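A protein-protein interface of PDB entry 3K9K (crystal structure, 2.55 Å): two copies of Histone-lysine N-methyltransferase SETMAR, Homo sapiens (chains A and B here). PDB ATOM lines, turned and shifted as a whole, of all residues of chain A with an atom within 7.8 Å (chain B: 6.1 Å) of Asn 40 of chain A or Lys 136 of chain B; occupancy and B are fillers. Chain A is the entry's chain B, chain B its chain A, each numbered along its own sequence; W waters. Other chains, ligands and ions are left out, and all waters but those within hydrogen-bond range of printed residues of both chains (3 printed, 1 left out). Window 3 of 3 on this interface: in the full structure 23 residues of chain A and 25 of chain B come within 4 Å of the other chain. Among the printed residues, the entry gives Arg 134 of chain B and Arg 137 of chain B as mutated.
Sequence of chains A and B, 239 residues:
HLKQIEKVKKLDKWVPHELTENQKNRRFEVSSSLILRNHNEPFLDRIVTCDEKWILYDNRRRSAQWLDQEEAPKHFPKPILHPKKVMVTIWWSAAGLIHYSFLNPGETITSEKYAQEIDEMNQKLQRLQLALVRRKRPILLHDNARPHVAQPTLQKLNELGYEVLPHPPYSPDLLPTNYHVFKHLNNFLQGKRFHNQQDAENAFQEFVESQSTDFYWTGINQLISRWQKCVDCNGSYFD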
ATOM      1  N   LEU A  34      -7.011 -20.885 -23.876  1.00  0.00           N
ATOM      2  CA  LEU A  34      -7.980 -21.455 -24.811  1.00  0.00           C
ATOM      3  C   LEU A  34      -8.495 -22.767 -24.253  1.00  0.00           C
ATOM      4  O   LEU A  34      -9.714 -22.969 -24.175  1.00  0.00           O
ATOM      5  CB  LEU A  34      -7.378 -21.639 -26.198  1.00  0.00           C
ATOM      6  CG  LEU A  34      -7.132 -20.310 -26.931  1.00  0.00           C
ATOM      7  CD1 LEU A  34      -6.461 -20.565 -28.239  1.00  0.00           C
ATOM      8  CD2 LEU A  34      -8.422 -19.521 -27.135  1.00  0.00           C
ATOM      9  N   ILE A  35      -7.565 -23.628 -23.825  1.00  0.00           N
ATOM     10  CA  ILE A  35      -7.912 -24.896 -23.200  1.00  0.00           C
ATOM     11  C   ILE A  35      -8.936 -24.700 -22.086  1.00  0.00           C
ATOM     12  O   ILE A  35      -9.962 -25.387 -22.030  1.00  0.00           O
ATOM     13  CB  ILE A  35      -6.676 -25.610 -22.644  1.00  0.00           C
ATOM     14  CG1 ILE A  35      -5.774 -26.061 -23.783  1.00  0.00           C
ATOM     15  CG2 ILE A  35      -7.080 -26.820 -21.810  1.00  0.00           C
ATOM     16  CD1 ILE A  35      -4.426 -26.567 -23.329  1.00  0.00           C
ATOM     17  N   LEU A  36      -8.659 -23.742 -21.206  1.00  0.00           N
ATOM     18  CA  LEU A  36      -9.567 -23.430 -20.111  1.00  0.00           C
ATOM     19  C   LEU A  36     -10.888 -22.875 -20.621  1.00  0.00           C
ATOM     20  O   LEU A  36     -11.953 -23.330 -20.198  1.00  0.00           O
ATOM     21  CB  LEU A  36      -8.909 -22.468 -19.121  1.00  0.00           C
ATOM     22  CG  LEU A  36      -7.847 -23.130 -18.242  1.00  0.00           C
ATOM     23  CD1 LEU A  36      -6.797 -22.132 -17.801  1.00  0.00           C
ATOM     24  CD2 LEU A  36      -8.512 -23.798 -17.050  1.00  0.00           C
ATOM     25  N   ARG A  37     -10.827 -21.910 -21.537  1.00  0.00           N
ATOM     26  CA  ARG A  37     -12.046 -21.282 -22.044  1.00  0.00           C
ATOM     27  C   ARG A  37     -13.002 -22.329 -22.590  1.00  0.00           C
ATOM     28  O   ARG A  37     -14.209 -22.301 -22.333  1.00  0.00           O
ATOM     29  CB  ARG A  37     -11.744 -20.243 -23.129  1.00  0.00           C
ATOM     30  CG  ARG A  37     -13.024 -19.621 -23.694  1.00  0.00           C
ATOM     31  CD  ARG A  37     -12.770 -18.436 -24.619  1.00  0.00           C
ATOM     32  NE  ARG A  37     -14.014 -18.050 -25.281  1.00  0.00           N
ATOM     33  CZ  ARG A  37     -14.112 -17.162 -26.265  1.00  0.00           C
ATOM     34  NH1 ARG A  37     -13.031 -16.532 -26.708  1.00  0.00           N
ATOM     35  NH2 ARG A  37     -15.302 -16.912 -26.808  1.00  0.00           N
ATOM     36  N   ASN A  38     -12.435 -23.267 -23.338  1.00  0.00           N
ATOM     37  CA  ASN A  38     -13.223 -24.241 -24.052  1.00  0.00           C
ATOM     38  C   ASN A  38     -13.796 -25.323 -23.144  1.00  0.00           C
ATOM     39  O   ASN A  38     -14.880 -25.854 -23.402  1.00  0.00           O
ATOM     40  CB  ASN A  38     -12.394 -24.867 -25.165  1.00  0.00           C
ATOM     41  CG  ASN A  38     -13.154 -25.922 -25.906  1.00  0.00           C
ATOM     42  OD1 ASN A  38     -12.890 -27.105 -25.745  1.00  0.00           O
ATOM     43  ND2 ASN A  38     -14.138 -25.506 -26.690  1.00  0.00           N
ATOM     44  N   HIS A  39     -13.071 -25.652 -22.084  1.00  0.00           N
ATOM     45  CA  HIS A  39     -13.563 -26.616 -21.112  1.00  0.00           C
ATOM     46  C   HIS A  39     -14.794 -26.095 -20.378  1.00  0.00           C
ATOM     47  O   HIS A  39     -15.723 -26.851 -20.061  1.00  0.00           O
ATOM     48  CB  HIS A  39     -12.472 -26.958 -20.114  1.00  0.00           C
ATOM     49  CG  HIS A  39     -12.871 -28.013 -19.131  1.00  0.00           C
ATOM     50  ND1 HIS A  39     -13.187 -27.726 -17.819  1.00  0.00           N
ATOM     51  CD2 HIS A  39     -13.003 -29.353 -19.266  1.00  0.00           C
ATOM     52  CE1 HIS A  39     -13.496 -28.844 -17.190  1.00  0.00           C
ATOM     53  NE2 HIS A  39     -13.396 -29.846 -18.046  1.00  0.00           N
ATOM     54  N   ASN A  40     -14.799 -24.795 -20.121  1.00  0.00           N
ATOM     55  CA  ASN A  40     -15.859 -24.178 -19.347  1.00  0.00           C
ATOM     56  C   ASN A  40     -16.957 -23.704 -20.282  1.00  0.00           C
ATOM     57  O   ASN A  40     -18.142 -23.944 -20.045  1.00  0.00           O
ATOM     58  CB  ASN A  40     -15.265 -23.045 -18.481  1.00  0.00           C
ATOM     59  CG  ASN A  40     -16.312 -22.101 -17.904  1.00  0.00           C
ATOM     60  OD1 ASN A  40     -17.103 -22.464 -17.022  1.00  0.00           O
ATOM     61  ND2 ASN A  40     -16.287 -20.861 -18.373  1.00  0.00           N
ATOM     62  N   GLU A  41     -16.569 -23.051 -21.369  1.00  0.00           N
ATOM     63  CA  GLU A  41     -17.554 -22.628 -22.354  1.00  0.00           C
ATOM     64  C   GLU A  41     -17.167 -23.017 -23.784  1.00  0.00           C
ATOM     65  O   GLU A  41     -16.696 -22.184 -24.551  1.00  0.00           O
ATOM     66  CB  GLU A  41     -17.837 -21.133 -22.216  1.00  0.00           C
ATOM     67  CG  GLU A  41     -18.905 -20.826 -21.151  1.00  0.00           C
ATOM     68  CD  GLU A  41     -19.136 -19.336 -20.939  1.00  0.00           C
ATOM     69  OE1 GLU A  41     -18.150 -18.566 -21.016  1.00  0.00           O
ATOM     70  OE2 GLU A  41     -20.298 -18.933 -20.690  1.00  0.00           O
ATOM     71  N   PRO A  42     -17.396 -24.293 -24.140  1.00  0.00           N
ATOM     72  CA  PRO A  42     -17.074 -24.949 -25.428  1.00  0.00           C
ATOM     73  C   PRO A  42     -17.410 -24.082 -26.642  1.00  0.00           C
ATOM     74  O   PRO A  42     -18.528 -23.575 -26.754  1.00  0.00           O
ATOM     75  CB  PRO A  42     -17.963 -26.205 -25.418  1.00  0.00           C
ATOM     76  CG  PRO A  42     -18.168 -26.496 -23.949  1.00  0.00           C
ATOM     77  CD  PRO A  42     -18.207 -25.159 -23.260  1.00  0.00           C
ATOM     78  N   PHE A  43     -16.450 -23.908 -27.544  1.00  0.00           N
ATOM     79  CA  PHE A  43     -16.654 -23.004 -28.671  1.00  0.00           C
ATOM     80  C   PHE A  43     -16.042 -23.552 -29.970  1.00  0.00           C
ATOM     81  O   PHE A  43     -16.133 -22.919 -31.012  1.00  0.00           O
ATOM     82  CB  PHE A  43     -16.071 -21.619 -28.339  1.00  0.00           C
ATOM     83  CG  PHE A  43     -14.590 -21.644 -28.117  1.00  0.00           C
ATOM     84  CD1 PHE A  43     -14.068 -21.658 -26.835  1.00  0.00           C
ATOM     85  CD2 PHE A  43     -13.723 -21.711 -29.193  1.00  0.00           C
ATOM     86  CE1 PHE A  43     -12.705 -21.703 -26.633  1.00  0.00           C
ATOM     87  CE2 PHE A  43     -12.373 -21.780 -28.998  1.00  0.00           C
ATOM     88  CZ  PHE A  43     -11.855 -21.770 -27.715  1.00  0.00           C
ATOM     89  N   PRO B  42     -21.688 -13.583 -21.290  1.00  0.00           N
ATOM     90  CA  PRO B  42     -21.294 -12.651 -20.225  1.00  0.00           C
ATOM     91  C   PRO B  42     -20.169 -13.210 -19.355  1.00  0.00           C
ATOM     92  O   PRO B  42     -20.285 -14.328 -18.856  1.00  0.00           O
ATOM     93  CB  PRO B  42     -22.565 -12.534 -19.381  1.00  0.00           C
ATOM     94  CG  PRO B  42     -23.658 -12.804 -20.313  1.00  0.00           C
ATOM     95  CD  PRO B  42     -23.141 -13.805 -21.310  1.00  0.00           C
ATOM     96  N   ARG B  46     -16.634 -12.312 -13.683  1.00  0.00           N
ATOM     97  CA  ARG B  46     -15.654 -13.358 -13.394  1.00  0.00           C
ATOM     98  C   ARG B  46     -14.259 -12.767 -13.457  1.00  0.00           C
ATOM     99  O   ARG B  46     -13.263 -13.450 -13.211  1.00  0.00           O
ATOM    100  CB  ARG B  46     -15.765 -14.504 -14.404  1.00  0.00           C
ATOM    101  CG  ARG B  46     -17.117 -15.168 -14.485  1.00  0.00           C
ATOM    102  CD  ARG B  46     -17.143 -16.089 -15.680  1.00  0.00           C
ATOM    103  NE  ARG B  46     -15.920 -16.888 -15.774  1.00  0.00           N
ATOM    104  CZ  ARG B  46     -15.540 -17.556 -16.865  1.00  0.00           C
ATOM    105  NH1 ARG B  46     -16.288 -17.513 -17.960  1.00  0.00           N
ATOM    106  NH2 ARG B  46     -14.414 -18.265 -16.869  1.00  0.00           N
ATOM    107  N   GLN B 129     -15.125 -16.246  -1.751  1.00  0.00           N
ATOM    108  CA  GLN B 129     -16.088 -16.983  -2.569  1.00  0.00           C
ATOM    109  C   GLN B 129     -16.654 -18.200  -1.862  1.00  0.00           C
ATOM    110  O   GLN B 129     -17.797 -18.590  -2.110  1.00  0.00           O
ATOM    111  CB  GLN B 129     -15.438 -17.444  -3.871  1.00  0.00           C
ATOM    112  CG  GLN B 129     -15.667 -16.529  -5.041  1.00  0.00           C
ATOM    113  CD  GLN B 129     -15.106 -17.106  -6.323  1.00  0.00           C
ATOM    114  OE1 GLN B 129     -14.108 -17.828  -6.305  1.00  0.00           O
ATOM    115  NE2 GLN B 129     -15.747 -16.797  -7.446  1.00  0.00           N
ATOM    116  N   ARG B 134     -22.247 -21.179  -6.858  1.00  0.00           N
ATOM    117  CA  ARG B 134     -21.193 -21.689  -7.700  1.00  0.00           C
ATOM    118  C   ARG B 134     -20.209 -20.568  -7.905  1.00  0.00           C
ATOM    119  O   ARG B 134     -20.552 -19.514  -8.443  1.00  0.00           O
ATOM    120  CB  ARG B 134     -21.706 -22.209  -9.043  1.00  0.00           C
ATOM    121  CG  ARG B 134     -20.901 -23.418  -9.520  1.00  0.00           C
ATOM    122  CD  ARG B 134     -20.753 -24.428  -8.357  1.00  0.00           C
ATOM    123  NE  ARG B 134     -19.728 -25.455  -8.576  1.00  0.00           N
ATOM    124  CZ  ARG B 134     -18.595 -25.577  -7.880  1.00  0.00           C
ATOM    125  NH1 ARG B 134     -18.303 -24.722  -6.907  1.00  0.00           N
ATOM    126  NH2 ARG B 134     -17.743 -26.558  -8.164  1.00  0.00           N
ATOM    127  N   ARG B 135     -18.997 -20.782  -7.414  1.00  0.00           N
ATOM    128  CA  ARG B 135     -17.892 -19.972  -7.848  1.00  0.00           C
ATOM    129  C   ARG B 135     -17.846 -20.253  -9.319  1.00  0.00           C
ATOM    130  O   ARG B 135     -17.945 -21.410  -9.729  1.00  0.00           O
ATOM    131  CB  ARG B 135     -16.581 -20.463  -7.249  1.00  0.00           C
ATOM    132  CG  ARG B 135     -16.534 -20.447  -5.754  1.00  0.00           C
ATOM    133  CD  ARG B 135     -17.294 -21.621  -5.190  1.00  0.00           C
ATOM    134  NE  ARG B 135     -17.244 -21.604  -3.739  1.00  0.00           N
ATOM    135  CZ  ARG B 135     -18.205 -22.073  -2.953  1.00  0.00           C
ATOM    136  NH1 ARG B 135     -18.059 -21.989  -1.642  1.00  0.00           N
ATOM    137  NH2 ARG B 135     -19.309 -22.611  -3.468  1.00  0.00           N
ATOM    138  N   LYS B 136     -17.714 -19.221 -10.132  1.00  0.00           N
ATOM    139  CA  LYS B 136     -17.255 -19.507 -11.467  1.00  0.00           C
ATOM    140  C   LYS B 136     -15.789 -19.123 -11.584  1.00  0.00           C
ATOM    141  O   LYS B 136     -15.235 -18.412 -10.735  1.00  0.00           O
ATOM    142  CB  LYS B 136     -18.128 -18.905 -12.573  1.00  0.00           C
ATOM    143  CG  LYS B 136     -17.860 -19.577 -13.924  1.00  0.00           C
ATOM    144  CD  LYS B 136     -19.138 -19.827 -14.706  1.00  0.00           C
ATOM    145  CE  LYS B 136     -18.866 -19.903 -16.203  1.00  0.00           C
ATOM    146  NZ  LYS B 136     -20.083 -19.529 -16.976  1.00  0.00           N
ATOM    147  N   ARG B 137     -15.175 -19.625 -12.641  1.00  0.00           N
ATOM    148  CA  ARG B 137     -13.738 -19.640 -12.762  1.00  0.00           C
ATOM    149  C   ARG B 137     -13.218 -18.286 -13.217  1.00  0.00           C
ATOM    150  O   ARG B 137     -13.733 -17.694 -14.160  1.00  0.00           O
ATOM    151  CB  ARG B 137     -13.372 -20.765 -13.711  1.00  0.00           C
ATOM    152  CG  ARG B 137     -14.460 -21.852 -13.683  1.00  0.00           C
ATOM    153  CD  ARG B 137     -13.947 -23.185 -14.177  1.00  0.00           C
ATOM    154  NE  ARG B 137     -13.647 -23.134 -15.605  1.00  0.00           N
ATOM    155  CZ  ARG B 137     -12.676 -23.827 -16.192  1.00  0.00           C
ATOM    156  NH1 ARG B 137     -11.891 -24.629 -15.469  1.00  0.00           N
ATOM    157  NH2 ARG B 137     -12.487 -23.706 -17.500  1.00  0.00           N
ATOM    158  N   PRO B 138     -12.187 -17.796 -12.528  1.00  0.00           N
ATOM    159  CA  PRO B 138     -11.688 -16.424 -12.606  1.00  0.00           C
ATOM    160  C   PRO B 138     -10.998 -16.095 -13.919  1.00  0.00           C
ATOM    161  O   PRO B 138     -10.206 -16.890 -14.422  1.00  0.00           O
ATOM    162  CB  PRO B 138     -10.646 -16.370 -11.477  1.00  0.00           C
ATOM    163  CG  PRO B 138     -10.870 -17.609 -10.658  1.00  0.00           C
ATOM    164  CD  PRO B 138     -11.389 -18.615 -11.604  1.00  0.00           C
ATOM    165  N   GLU B 163      -7.894 -18.290 -16.565  1.00  0.00           N
ATOM    166  CA  GLU B 163      -7.960 -17.789 -17.917  1.00  0.00           C
ATOM    167  C   GLU B 163      -7.382 -16.378 -17.908  1.00  0.00           C
ATOM    168  O   GLU B 163      -7.467 -15.665 -16.907  1.00  0.00           O
ATOM    169  CB  GLU B 163      -9.418 -17.748 -18.343  1.00  0.00           C
ATOM    170  CG  GLU B 163      -9.685 -18.095 -19.782  1.00  0.00           C
ATOM    171  CD  GLU B 163     -11.181 -18.133 -20.058  1.00  0.00           C
ATOM    172  OE1 GLU B 163     -11.891 -18.947 -19.399  1.00  0.00           O
ATOM    173  OE2 GLU B 163     -11.639 -17.336 -20.915  1.00  0.00           O
HETATM  174  O   HOH W   1     -14.325 -19.179 -19.982  1.00  0.00           O
HETATM  175  O   HOH W   2     -20.098 -22.507 -17.985  1.00  0.00           O
HETATM  176  O   HOH W   3     -18.350 -16.486 -18.981  1.00  0.00           O
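The guanidinium group (NH1) of Arg 46 of chain B sits close to the side-chain amide nitrogen (ND2) of Asn 40 of chain A, at 3.4 Å.
OE1 of Glu 41 of chain A lies within salt-bridge range of NH1 of Arg 46 of chain B (3.7 Å).
The side-chain amino group (NZ) of Lys 136 of chain B is in salt-bridge range of the side-chain carboxylate (OE2) of Glu 41 of chain A, at 3.8 Å.
The guanidinium group (NH2) of Arg 137 of chain B lies within hydrogen-bond range of the backbone carbonyl oxygen (O) of Leu 36 of chain A, 2.8 Å away.
O of Arg 137 of chain B is in hydrogen-bond range of NE of Arg 46 of chain B, at 2.8 Å.
The guanidinium group (NH2) of Arg 46 of chain B is in salt-bridge range of the side-chain carboxylate (OE1) of Glu 163 of chain B (3.6 Å).
N of Glu 163 of chain B is in hydrogen-bond range of O of Pro 138 of chain B (3.4 Å).
Arg 37 of chain A touches Glu 163 of chain B (CA to OE1, 3.5 Å).
Lys 136 of chain B touches Asn 40 of chain A (CE to OD1, 3.2 Å).
Asn 40 of chain A touches Arg 137 of chain B.
Of the printed residues of chain B, Leu 36 of chain A touches Arg 137.
Printed residues of chain B within 4 Å of Arg 37 of chain A: Glu 163.
Printed residues of chain B within 4 Å of Asn 40 of chain A: Arg 46 (3.4 Å), Lys 136 (3.2 Å) and Arg 137 (3.0 Å).
Of the printed residues of chain B, Glu 41 of chain A touches Arg 46 (3.7 Å) and Lys 136 (3.8 Å).
Pro 42 of chain A touches none of the printed residues of chain B.
Of the printed residues of chain A, Arg 46 of chain B touches Asn 40 (3.4 Å) and Glu 41 (3.7 Å).
Of chain A, only Asn 40 and Glu 41 come within 4 Å of Lys 136 of chain B.
Printed residues of chain A within 4 Å of Glu 163 of chain B: Arg 37 (3.5 Å).
Of the 10 printed residues of chain A, 4 touch a printed residue of chain B.
Of the 9 printed residues of chain B, 4 touch a printed residue of chain A.
Among the printed residues, 7 pairs touch across the chains.
Position printed for both chains: 42.
Of the 7 pairs that touch across the chains among the printed residues, none has its exchanged pair printed and touching as well.
Water W1 lies within hydrogen-bond range of the side-chain carboxylate (OE1) of Glu 163 of chain B, the side-chain amide nitrogen (ND2) of Asn 40 of chain A and the guanidinium group (NH2) of Arg 46 of chain B.
Water W3 lies within hydrogen-bond range of NH1 of Arg 46 of chain B, O of Pro 42 of chain B and OE1 of Glu 41 of chain A.
Water W2 lies within hydrogen-bond range of NZ of Lys 136 of chain B (3.1 Å) and OD1 of Asn 40 of chain A (3.1 Å).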
